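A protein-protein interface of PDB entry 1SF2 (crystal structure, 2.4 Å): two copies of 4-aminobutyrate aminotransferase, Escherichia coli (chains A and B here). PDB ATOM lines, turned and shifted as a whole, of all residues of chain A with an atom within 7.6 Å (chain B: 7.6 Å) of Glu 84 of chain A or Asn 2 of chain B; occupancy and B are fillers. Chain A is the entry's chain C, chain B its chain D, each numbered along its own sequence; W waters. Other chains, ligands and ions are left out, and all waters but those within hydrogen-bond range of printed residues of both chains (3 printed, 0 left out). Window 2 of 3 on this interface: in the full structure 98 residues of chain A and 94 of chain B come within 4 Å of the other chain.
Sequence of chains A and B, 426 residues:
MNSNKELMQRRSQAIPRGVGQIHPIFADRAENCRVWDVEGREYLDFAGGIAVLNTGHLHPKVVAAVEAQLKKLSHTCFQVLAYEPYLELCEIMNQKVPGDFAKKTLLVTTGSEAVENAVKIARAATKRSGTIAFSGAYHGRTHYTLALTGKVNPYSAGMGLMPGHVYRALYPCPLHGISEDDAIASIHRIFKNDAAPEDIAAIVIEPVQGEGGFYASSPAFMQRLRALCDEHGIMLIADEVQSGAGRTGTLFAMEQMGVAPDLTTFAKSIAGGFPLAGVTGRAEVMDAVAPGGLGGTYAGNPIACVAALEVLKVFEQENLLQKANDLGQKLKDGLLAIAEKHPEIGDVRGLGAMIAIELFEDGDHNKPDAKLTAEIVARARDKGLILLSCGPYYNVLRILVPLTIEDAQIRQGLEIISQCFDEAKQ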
ATOM      1  N   GLN A  69      19.471  -5.286  -9.855  1.00  0.00           N
ATOM      2  CA  GLN A  69      18.463  -5.404 -10.904  1.00  0.00           C
ATOM      3  C   GLN A  69      18.251  -4.074 -11.621  1.00  0.00           C
ATOM      4  O   GLN A  69      17.981  -4.045 -12.824  1.00  0.00           O
ATOM      5  CB  GLN A  69      17.135  -5.879 -10.309  1.00  0.00           C
ATOM      6  CG  GLN A  69      16.020  -6.113 -11.327  1.00  0.00           C
ATOM      7  CD  GLN A  69      16.366  -7.181 -12.367  1.00  0.00           C
ATOM      8  OE1 GLN A  69      17.106  -8.128 -12.081  1.00  0.00           O
ATOM      9  NE2 GLN A  69      15.814  -7.039 -13.571  1.00  0.00           N
ATOM     10  N   PHE A  78       5.711  -8.855 -17.926  1.00  0.00           N
ATOM     11  CA  PHE A  78       5.916 -10.291 -18.036  1.00  0.00           C
ATOM     12  C   PHE A  78       5.147 -11.026 -19.139  1.00  0.00           C
ATOM     13  O   PHE A  78       5.731 -11.816 -19.889  1.00  0.00           O
ATOM     14  CB  PHE A  78       5.605 -10.948 -16.699  1.00  0.00           C
ATOM     15  CG  PHE A  78       5.977 -12.403 -16.648  1.00  0.00           C
ATOM     16  CD1 PHE A  78       7.272 -12.792 -16.310  1.00  0.00           C
ATOM     17  CD2 PHE A  78       5.025 -13.389 -16.924  1.00  0.00           C
ATOM     18  CE1 PHE A  78       7.611 -14.147 -16.240  1.00  0.00           C
ATOM     19  CE2 PHE A  78       5.359 -14.755 -16.859  1.00  0.00           C
ATOM     20  CZ  PHE A  78       6.652 -15.129 -16.515  1.00  0.00           C
ATOM     21  N   ALA A  82       8.988 -12.180 -20.916  1.00  0.00           N
ATOM     22  CA  ALA A  82       9.234 -12.630 -19.545  1.00  0.00           C
ATOM     23  C   ALA A  82      10.639 -12.352 -19.015  1.00  0.00           C
ATOM     24  O   ALA A  82      11.514 -11.858 -19.739  1.00  0.00           O
ATOM     25  CB  ALA A  82       8.914 -14.118 -19.418  1.00  0.00           C
ATOM     26  N   TYR A  83      10.838 -12.669 -17.743  1.00  0.00           N
ATOM     27  CA  TYR A  83      12.122 -12.486 -17.089  1.00  0.00           C
ATOM     28  C   TYR A  83      12.181 -13.442 -15.909  1.00  0.00           C
ATOM     29  O   TYR A  83      11.152 -13.773 -15.312  1.00  0.00           O
ATOM     30  CB  TYR A  83      12.323 -11.015 -16.650  1.00  0.00           C
ATOM     31  CG  TYR A  83      11.074 -10.328 -16.131  1.00  0.00           C
ATOM     32  CD1 TYR A  83      10.743 -10.361 -14.769  1.00  0.00           C
ATOM     33  CD2 TYR A  83      10.202  -9.690 -17.009  1.00  0.00           C
ATOM     34  CE1 TYR A  83       9.573  -9.784 -14.300  1.00  0.00           C
ATOM     35  CE2 TYR A  83       9.024  -9.108 -16.553  1.00  0.00           C
ATOM     36  CZ  TYR A  83       8.710  -9.155 -15.195  1.00  0.00           C
ATOM     37  OH  TYR A  83       7.542  -8.564 -14.741  1.00  0.00           O
ATOM     38  N   GLU A  84      13.387 -13.890 -15.586  1.00  0.00           N
ATOM     39  CA  GLU A  84      13.597 -14.861 -14.521  1.00  0.00           C
ATOM     40  C   GLU A  84      13.141 -14.591 -13.090  1.00  0.00           C
ATOM     41  O   GLU A  84      12.583 -15.488 -12.445  1.00  0.00           O
ATOM     42  CB  GLU A  84      15.071 -15.282 -14.494  1.00  0.00           C
ATOM     43  CG  GLU A  84      15.283 -16.664 -15.078  1.00  0.00           C
ATOM     44  CD  GLU A  84      16.693 -17.201 -14.863  1.00  0.00           C
ATOM     45  OE1 GLU A  84      17.639 -16.667 -15.498  1.00  0.00           O
ATOM     46  OE2 GLU A  84      16.839 -18.159 -14.056  1.00  0.00           O
ATOM     47  N   PRO A  85      13.389 -13.378 -12.561  1.00  0.00           N
ATOM     48  CA  PRO A  85      12.964 -13.103 -11.184  1.00  0.00           C
ATOM     49  C   PRO A  85      11.501 -13.435 -10.929  1.00  0.00           C
ATOM     50  O   PRO A  85      11.137 -13.884  -9.850  1.00  0.00           O
ATOM     51  CB  PRO A  85      13.268 -11.613 -11.015  1.00  0.00           C
ATOM     52  CG  PRO A  85      14.479 -11.437 -11.906  1.00  0.00           C
ATOM     53  CD  PRO A  85      14.081 -12.210 -13.140  1.00  0.00           C
ATOM     54  N   TYR A  86      10.665 -13.205 -11.929  1.00  0.00           N
ATOM     55  CA  TYR A  86       9.245 -13.491 -11.804  1.00  0.00           C
ATOM     56  C   TYR A  86       9.060 -15.015 -11.675  1.00  0.00           C
ATOM     57  O   TYR A  86       8.466 -15.504 -10.711  1.00  0.00           O
ATOM     58  CB  TYR A  86       8.525 -12.946 -13.041  1.00  0.00           C
ATOM     59  CG  TYR A  86       7.026 -13.116 -13.045  1.00  0.00           C
ATOM     60  CD1 TYR A  86       6.190 -12.015 -13.246  1.00  0.00           C
ATOM     61  CD2 TYR A  86       6.437 -14.372 -12.886  1.00  0.00           C
ATOM     62  CE1 TYR A  86       4.811 -12.160 -13.291  1.00  0.00           C
ATOM     63  CE2 TYR A  86       5.044 -14.525 -12.930  1.00  0.00           C
ATOM     64  CZ  TYR A  86       4.245 -13.411 -13.135  1.00  0.00           C
ATOM     65  OH  TYR A  86       2.878 -13.527 -13.206  1.00  0.00           O
ATOM     66  N   LEU A  87       9.591 -15.750 -12.652  1.00  0.00           N
ATOM     67  CA  LEU A  87       9.515 -17.208 -12.682  1.00  0.00           C
ATOM     68  C   LEU A  87      10.068 -17.843 -11.407  1.00  0.00           C
ATOM     69  O   LEU A  87       9.418 -18.673 -10.783  1.00  0.00           O
ATOM     70  CB  LEU A  87      10.286 -17.738 -13.900  1.00  0.00           C
ATOM     71  CG  LEU A  87      10.634 -19.235 -13.918  1.00  0.00           C
ATOM     72  CD1 LEU A  87       9.356 -20.078 -13.828  1.00  0.00           C
ATOM     73  CD2 LEU A  87      11.420 -19.568 -15.182  1.00  0.00           C
ATOM     74  N   GLU A  88      11.272 -17.445 -11.017  1.00  0.00           N
ATOM     75  CA  GLU A  88      11.895 -18.005  -9.825  1.00  0.00           C
ATOM     76  C   GLU A  88      11.071 -17.826  -8.547  1.00  0.00           C
ATOM     77  O   GLU A  88      10.984 -18.746  -7.709  1.00  0.00           O
ATOM     78  CB  GLU A  88      13.289 -17.406  -9.604  1.00  0.00           C
ATOM     79  CG  GLU A  88      14.047 -18.141  -8.512  1.00  0.00           C
ATOM     80  CD  GLU A  88      15.416 -17.557  -8.208  1.00  0.00           C
ATOM     81  OE1 GLU A  88      15.963 -16.801  -9.047  1.00  0.00           O
ATOM     82  OE2 GLU A  88      15.949 -17.883  -7.123  1.00  0.00           O
ATOM     83  N   LEU A  89      10.474 -16.649  -8.391  1.00  0.00           N
ATOM     84  CA  LEU A  89       9.690 -16.369  -7.204  1.00  0.00           C
ATOM     85  C   LEU A  89       8.465 -17.258  -7.177  1.00  0.00           C
ATOM     86  O   LEU A  89       8.088 -17.762  -6.109  1.00  0.00           O
ATOM     87  CB  LEU A  89       9.279 -14.892  -7.156  1.00  0.00           C
ATOM     88  CG  LEU A  89       8.445 -14.491  -5.934  1.00  0.00           C
ATOM     89  CD1 LEU A  89       9.241 -14.742  -4.653  1.00  0.00           C
ATOM     90  CD2 LEU A  89       8.038 -13.036  -6.045  1.00  0.00           C
ATOM     91  N   CYS A  90       7.841 -17.462  -8.340  1.00  0.00           N
ATOM     92  CA  CYS A  90       6.652 -18.316  -8.388  1.00  0.00           C
ATOM     93  C   CYS A  90       7.059 -19.713  -7.938  1.00  0.00           C
ATOM     94  O   CYS A  90       6.390 -20.331  -7.106  1.00  0.00           O
ATOM     95  CB  CYS A  90       6.065 -18.373  -9.799  1.00  0.00           C
ATOM     96  SG  CYS A  90       5.325 -16.830 -10.369  1.00  0.00           S
ATOM     97  N   GLU A  91       8.175 -20.203  -8.466  1.00  0.00           N
ATOM     98  CA  GLU A  91       8.653 -21.533  -8.093  1.00  0.00           C
ATOM     99  C   GLU A  91       8.851 -21.649  -6.587  1.00  0.00           C
ATOM    100  O   GLU A  91       8.444 -22.627  -5.964  1.00  0.00           O
ATOM    101  CB  GLU A  91       9.956 -21.847  -8.820  1.00  0.00           C
ATOM    102  CG  GLU A  91       9.788 -21.901 -10.323  1.00  0.00           C
ATOM    103  CD  GLU A  91      11.095 -22.158 -11.029  1.00  0.00           C
ATOM    104  OE1 GLU A  91      12.127 -21.647 -10.538  1.00  0.00           O
ATOM    105  OE2 GLU A  91      11.091 -22.852 -12.074  1.00  0.00           O
ATOM    106  N   CYS A 305      10.424  -8.191  -7.584  1.00  0.00           N
ATOM    107  CA  CYS A 305      10.661  -9.634  -7.545  1.00  0.00           C
ATOM    108  C   CYS A 305      11.989  -9.985  -6.864  1.00  0.00           C
ATOM    109  O   CYS A 305      12.013 -10.821  -5.951  1.00  0.00           O
ATOM    110  CB  CYS A 305      10.658 -10.219  -8.951  1.00  0.00           C
ATOM    111  SG  CYS A 305       9.059 -10.313  -9.762  1.00  0.00           S
ATOM    112  N   VAL A 306      13.090  -9.370  -7.297  1.00  0.00           N
ATOM    113  CA  VAL A 306      14.372  -9.681  -6.673  1.00  0.00           C
ATOM    114  C   VAL A 306      14.331  -9.238  -5.209  1.00  0.00           C
ATOM    115  O   VAL A 306      14.978  -9.846  -4.349  1.00  0.00           O
ATOM    116  CB  VAL A 306      15.578  -9.001  -7.403  1.00  0.00           C
ATOM    117  CG1 VAL A 306      15.515  -9.306  -8.902  1.00  0.00           C
ATOM    118  CG2 VAL A 306      15.599  -7.507  -7.140  1.00  0.00           C
ATOM    119  N   LEU A 309      12.590 -12.096  -3.559  1.00  0.00           N
ATOM    120  CA  LEU A 309      13.484 -13.237  -3.513  1.00  0.00           C
ATOM    121  C   LEU A 309      14.541 -13.032  -2.425  1.00  0.00           C
ATOM    122  O   LEU A 309      14.936 -13.979  -1.756  1.00  0.00           O
ATOM    123  CB  LEU A 309      14.163 -13.433  -4.877  1.00  0.00           C
ATOM    124  CG  LEU A 309      13.249 -13.905  -6.016  1.00  0.00           C
ATOM    125  CD1 LEU A 309      13.943 -13.707  -7.336  1.00  0.00           C
ATOM    126  CD2 LEU A 309      12.862 -15.368  -5.806  1.00  0.00           C
ATOM    127  N   ASN B   2      21.632 -18.780 -20.326  1.00  0.00           N
ATOM    128  CA  ASN B   2      20.485 -19.721 -20.147  1.00  0.00           C
ATOM    129  C   ASN B   2      19.861 -20.069 -21.506  1.00  0.00           C
ATOM    130  O   ASN B   2      20.526 -20.029 -22.542  1.00  0.00           O
ATOM    131  CB  ASN B   2      19.430 -19.078 -19.231  1.00  0.00           C
ATOM    132  CG  ASN B   2      18.668 -20.103 -18.388  1.00  0.00           C
ATOM    133  OD1 ASN B   2      18.109 -21.076 -18.914  1.00  0.00           O
ATOM    134  ND2 ASN B   2      18.638 -19.879 -17.068  1.00  0.00           N
ATOM    135  N   SER B   3      18.583 -20.429 -21.489  1.00  0.00           N
ATOM    136  CA  SER B   3      17.851 -20.762 -22.703  1.00  0.00           C
ATOM    137  C   SER B   3      16.415 -20.261 -22.556  1.00  0.00           C
ATOM    138  O   SER B   3      15.770 -20.516 -21.540  1.00  0.00           O
ATOM    139  CB  SER B   3      17.831 -22.275 -22.923  1.00  0.00           C
ATOM    140  OG  SER B   3      16.823 -22.639 -23.854  1.00  0.00           O
ATOM    141  N   ASN B   4      15.919 -19.544 -23.557  1.00  0.00           N
ATOM    142  CA  ASN B   4      14.551 -19.065 -23.506  1.00  0.00           C
ATOM    143  C   ASN B   4      13.615 -20.251 -23.309  1.00  0.00           C
ATOM    144  O   ASN B   4      12.786 -20.252 -22.403  1.00  0.00           O
ATOM    145  CB  ASN B   4      14.180 -18.338 -24.801  1.00  0.00           C
ATOM    146  CG  ASN B   4      14.803 -16.960 -24.893  1.00  0.00           C
ATOM    147  OD1 ASN B   4      14.729 -16.171 -23.947  1.00  0.00           O
ATOM    148  ND2 ASN B   4      15.411 -16.656 -26.036  1.00  0.00           N
ATOM    149  N   LYS B   5      13.767 -21.268 -24.157  1.00  0.00           N
ATOM    150  CA  LYS B   5      12.920 -22.452 -24.097  1.00  0.00           C
ATOM    151  C   LYS B   5      12.944 -23.157 -22.746  1.00  0.00           C
ATOM    152  O   LYS B   5      11.904 -23.616 -22.258  1.00  0.00           O
ATOM    153  CB  LYS B   5      13.310 -23.421 -25.208  1.00  0.00           C
ATOM    154  CG  LYS B   5      13.007 -22.894 -26.599  1.00  0.00           C
ATOM    155  CD  LYS B   5      13.543 -23.827 -27.667  1.00  0.00           C
ATOM    156  CE  LYS B   5      13.414 -23.201 -29.039  1.00  0.00           C
ATOM    157  NZ  LYS B   5      11.993 -22.865 -29.291  1.00  0.00           N
ATOM    158  N   GLU B   6      14.121 -23.249 -22.140  1.00  0.00           N
ATOM    159  CA  GLU B   6      14.212 -23.882 -20.834  1.00  0.00           C
ATOM    160  C   GLU B   6      13.379 -23.082 -19.828  1.00  0.00           C
ATOM    161  O   GLU B   6      12.632 -23.654 -19.021  1.00  0.00           O
ATOM    162  CB  GLU B   6      15.655 -23.938 -20.353  1.00  0.00           C
ATOM    163  CG  GLU B   6      15.801 -24.750 -19.097  1.00  0.00           C
ATOM    164  CD  GLU B   6      17.145 -24.572 -18.440  1.00  0.00           C
ATOM    165  OE1 GLU B   6      18.181 -24.737 -19.130  1.00  0.00           O
ATOM    166  OE2 GLU B   6      17.163 -24.267 -17.226  1.00  0.00           O
ATOM    167  N   LEU B   7      13.518 -21.757 -19.869  1.00  0.00           N
ATOM    168  CA  LEU B   7      12.754 -20.895 -18.972  1.00  0.00           C
ATOM    169  C   LEU B   7      11.245 -21.038 -19.235  1.00  0.00           C
ATOM    170  O   LEU B   7      10.450 -21.035 -18.296  1.00  0.00           O
ATOM    171  CB  LEU B   7      13.214 -19.433 -19.106  1.00  0.00           C
ATOM    172  CG  LEU B   7      14.645 -19.275 -18.559  1.00  0.00           C
ATOM    173  CD1 LEU B   7      15.159 -17.868 -18.803  1.00  0.00           C
ATOM    174  CD2 LEU B   7      14.675 -19.619 -17.065  1.00  0.00           C
ATOM    175  N   MET B   8      10.858 -21.187 -20.502  1.00  0.00           N
ATOM    176  CA  MET B   8       9.449 -21.379 -20.858  1.00  0.00           C
ATOM    177  C   MET B   8       8.895 -22.676 -20.258  1.00  0.00           C
ATOM    178  O   MET B   8       7.745 -22.715 -19.806  1.00  0.00           O
ATOM    179  CB  MET B   8       9.262 -21.408 -22.375  1.00  0.00           C
ATOM    180  CG  MET B   8       9.303 -20.038 -23.029  1.00  0.00           C
ATOM    181  SD  MET B   8       8.021 -18.885 -22.385  1.00  0.00           S
ATOM    182  CE  MET B   8       6.556 -19.629 -23.055  1.00  0.00           C
ATOM    183  N   ARG B  10       9.909 -24.177 -17.492  1.00  0.00           N
ATOM    184  CA  ARG B  10       9.759 -23.969 -16.057  1.00  0.00           C
ATOM    185  C   ARG B  10       8.506 -23.140 -15.828  1.00  0.00           C
ATOM    186  O   ARG B  10       7.780 -23.348 -14.855  1.00  0.00           O
ATOM    187  CB  ARG B  10      10.979 -23.228 -15.483  1.00  0.00           C
ATOM    188  CG  ARG B  10      12.212 -24.098 -15.314  1.00  0.00           C
ATOM    189  CD  ARG B  10      13.461 -23.276 -15.019  1.00  0.00           C
ATOM    190  NE  ARG B  10      13.364 -22.528 -13.774  1.00  0.00           N
ATOM    191  CZ  ARG B  10      14.231 -21.588 -13.408  1.00  0.00           C
ATOM    192  NH1 ARG B  10      15.264 -21.286 -14.189  1.00  0.00           N
ATOM    193  NH2 ARG B  10      14.047 -20.917 -12.289  1.00  0.00           N
ATOM    194  N   ILE B  15       3.788 -21.525 -13.380  1.00  0.00           N
ATOM    195  CA  ILE B  15       2.833 -20.451 -13.617  1.00  0.00           C
ATOM    196  C   ILE B  15       1.607 -20.920 -14.401  1.00  0.00           C
ATOM    197  O   ILE B  15       1.724 -21.668 -15.370  1.00  0.00           O
ATOM    198  CB  ILE B  15       3.552 -19.290 -14.358  1.00  0.00           C
ATOM    199  CG1 ILE B  15       4.748 -18.838 -13.513  1.00  0.00           C
ATOM    200  CG2 ILE B  15       2.586 -18.119 -14.630  1.00  0.00           C
ATOM    201  CD1 ILE B  15       5.638 -17.789 -14.169  1.00  0.00           C
ATOM    202  N   PHE B  26      12.725 -14.566 -22.676  1.00  0.00           N
ATOM    203  CA  PHE B  26      13.055 -14.052 -21.352  1.00  0.00           C
ATOM    204  C   PHE B  26      14.129 -12.981 -21.434  1.00  0.00           C
ATOM    205  O   PHE B  26      15.278 -13.259 -21.779  1.00  0.00           O
ATOM    206  CB  PHE B  26      13.530 -15.175 -20.414  1.00  0.00           C
ATOM    207  CG  PHE B  26      12.410 -15.947 -19.771  1.00  0.00           C
ATOM    208  CD1 PHE B  26      11.577 -16.768 -20.538  1.00  0.00           C
ATOM    209  CD2 PHE B  26      12.183 -15.854 -18.400  1.00  0.00           C
ATOM    210  CE1 PHE B  26      10.529 -17.490 -19.942  1.00  0.00           C
ATOM    211  CE2 PHE B  26      11.142 -16.568 -17.789  1.00  0.00           C
ATOM    212  CZ  PHE B  26      10.311 -17.392 -18.567  1.00  0.00           C
ATOM    213  N   ALA B  27      13.744 -11.755 -21.104  1.00  0.00           N
ATOM    214  CA  ALA B  27      14.666 -10.634 -21.122  1.00  0.00           C
ATOM    215  C   ALA B  27      15.621 -10.699 -19.938  1.00  0.00           C
ATOM    216  O   ALA B  27      15.282 -11.230 -18.874  1.00  0.00           O
ATOM    217  CB  ALA B  27      13.886  -9.307 -21.093  1.00  0.00           C
ATOM    218  N   ASP B  28      16.825 -10.158 -20.134  1.00  0.00           N
ATOM    219  CA  ASP B  28      17.833 -10.105 -19.075  1.00  0.00           C
ATOM    220  C   ASP B  28      18.205  -8.644 -18.764  1.00  0.00           C
ATOM    221  O   ASP B  28      18.223  -8.228 -17.606  1.00  0.00           O
ATOM    222  CB  ASP B  28      19.095 -10.861 -19.485  1.00  0.00           C
ATOM    223  CG  ASP B  28      20.139 -10.866 -18.385  1.00  0.00           C
ATOM    224  OD1 ASP B  28      19.886 -11.483 -17.327  1.00  0.00           O
ATOM    225  OD2 ASP B  28      21.202 -10.241 -18.569  1.00  0.00           O
ATOM    226  N   ASP B  37      18.028 -10.828 -24.435  1.00  0.00           N
ATOM    227  CA  ASP B  37      17.448 -11.936 -23.682  1.00  0.00           C
ATOM    228  C   ASP B  37      18.520 -12.758 -22.995  1.00  0.00           C
ATOM    229  O   ASP B  37      19.700 -12.424 -23.064  1.00  0.00           O
ATOM    230  CB  ASP B  37      16.575 -12.830 -24.580  1.00  0.00           C
ATOM    231  CG  ASP B  37      17.361 -13.527 -25.695  1.00  0.00           C
ATOM    232  OD1 ASP B  37      18.605 -13.698 -25.575  1.00  0.00           O
ATOM    233  OD2 ASP B  37      16.705 -13.923 -26.689  1.00  0.00           O
ATOM    234  N   VAL B  38      18.118 -13.826 -22.317  1.00  0.00           N
ATOM    235  CA  VAL B  38      19.081 -14.660 -21.609  1.00  0.00           C
ATOM    236  C   VAL B  38      20.073 -15.360 -22.536  1.00  0.00           C
ATOM    237  O   VAL B  38      21.117 -15.822 -22.104  1.00  0.00           O
ATOM    238  CB  VAL B  38      18.368 -15.723 -20.728  1.00  0.00           C
ATOM    239  CG1 VAL B  38      17.551 -15.022 -19.621  1.00  0.00           C
ATOM    240  CG2 VAL B  38      17.465 -16.605 -21.597  1.00  0.00           C
ATOM    241  N   GLU B  39      19.754 -15.437 -23.818  1.00  0.00           N
ATOM    242  CA  GLU B  39      20.654 -16.091 -24.763  1.00  0.00           C
ATOM    243  C   GLU B  39      21.593 -15.076 -25.394  1.00  0.00           C
ATOM    244  O   GLU B  39      22.329 -15.404 -26.318  1.00  0.00           O
ATOM    245  CB  GLU B  39      19.847 -16.808 -25.850  1.00  0.00           C
ATOM    246  CG  GLU B  39      19.152 -18.064 -25.347  1.00  0.00           C
ATOM    247  CD  GLU B  39      18.220 -18.678 -26.375  1.00  0.00           C
ATOM    248  OE1 GLU B  39      18.454 -18.481 -27.587  1.00  0.00           O
ATOM    249  OE2 GLU B  39      17.262 -19.372 -25.970  1.00  0.00           O
ATOM    250  N   GLY B  40      21.551 -13.841 -24.895  1.00  0.00           N
ATOM    251  CA  GLY B  40      22.412 -12.790 -25.412  1.00  0.00           C
ATOM    252  C   GLY B  40      21.933 -12.140 -26.697  1.00  0.00           C
ATOM    253  O   GLY B  40      22.621 -11.299 -27.281  1.00  0.00           O
HETATM  254  O   HOH W   1      18.083 -13.751 -16.214  1.00  0.00           O
HETATM  255  O   HOH W   2       9.126 -24.443 -12.748  1.00  0.00           O
HETATM  256  O   HOH W   3      15.326 -13.383 -17.330  1.00  0.00           O
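No position is printed for both chains. Of the 15 pairs that touch across the chains among the printed residues, none has its exchanged pair printed and touching as well.
CD1 of Ile 15 of chain B touches CZ of Phe 78 of chain A, 3.7 Å away. Ala 82 of chain A touches Phe 26 of chain B. Tyr 83 of chain A touches Phe 26 of chain B (C to CD2, 3.5 Å). Tyr 83 of chain A touches Ala 27 of chain B (CB to O, 3.7 Å). Asn 2 of chain B touches Glu 84 of chain A (ND2 to OE1, 3.7 Å). Phe 26 of chain B touches Glu 84 of chain A. Tyr 86 of chain A touches Ile 15 of chain B (CE2 to CD1, 3.5 Å). CD2 of Leu 87 of chain A touches O of Leu 7 of chain B, 3.6 Å away. Leu 87 of chain A touches Arg 10 of chain B. CD2 of Leu 87 of chain A touches CE2 of Phe 26 of chain B, at 3.98 Å.
SG of Cys 90 of chain A lies within hydrogen-bond range of O of Tyr 86 of chain A, 3.4 Å away. N of Asn 2 of chain B is in hydrogen-bond range of O of Val 38 of chain B (3.5 Å). The side-chain amide oxygen of Asn 4 of chain B sits at hydrogen-bond distance from the backbone NH of Phe 26 of chain B (2.9 Å). The backbone carbonyl oxygen (O) of Phe 26 of chain B lies within hydrogen-bond range of the backbone NH (N) of Val 38 of chain B (2.9 Å).
Of the printed residues of chain B, Phe 78 of chain A touches Ile 15 (3.7 Å). Of the printed residues of chain B, Ala 82 of chain A touches Phe 26 and Ala 27. Of chain B, only Asn 2, Leu 7, Arg 10 and Phe 26 come within 4 Å of Glu 84 of chain A. Of the printed residues of chain B, Cys 90 of chain A touches Ile 15. Of chain A, only Glu 84 (3.7 Å) comes within 4 Å of Asn 2 of chain B. Printed residues of chain A within 4 Å of Ile 15 of chain B: Phe 78 (3.7 Å), Tyr 86 (3.5 Å) and Cys 90 (3.8 Å). The nearest residue of chain B that does not touch Glu 84 of chain A is Val 38 of chain B (4.4 Å). The nearest residue of chain A that does not touch Asn 2 of chain B is Leu 87 of chain A (7.5 Å).
Water W2 bridges the side-chain carboxylate (OE2) of Glu 91 of chain A (2.6 Å) and the backbone carbonyl oxygen (O) of Arg 10 of chain B (2.7 Å). Water W3 bridges O of Ala 27 of chain B and N of Glu 84 of chain A. Water W1 lies within hydrogen-bond range of the side-chain carboxylate of Glu 84 of chain A and the side-chain carboxylate of Asp 28 of chain B.
Of the 15 printed residues of chain A, 8 touch a printed residue of chain B. Printed residues of chain A that touch a printed residue of chain B: Phe 78, Ala 82, Tyr 83, Glu 84, Tyr 86, Leu 87, Cys 90 and Glu 91. Of the 16 printed residues of chain B, 6 touch a printed residue of chain A. Along chain B the printed residues that touch a printed residue of chain A span positions 2 to 27. Among the printed residues, Asp or Glu carboxylates within 4 Å of a Lys or Arg side-chain nitrogen of the other chain: Glu 84 of chain A with Arg 10 of chain B and Glu 91 of chain A with Arg 10 of chain B.
The backbone carbonyl oxygen of Ala 82 of chain A is in hydrogen-bond range of the backbone NH of Ala 27 of chain B (2.6 Å). NH1 of Arg 10 of chain B is in salt-bridge range of OE2 of Glu 84 of chain A (3.5 Å). The side-chain carboxylate (OE1) of Glu 91 of chain A lies within salt-bridge range of the guanidinium group (NH2) of Arg 10 of chain B (2.7 Å).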
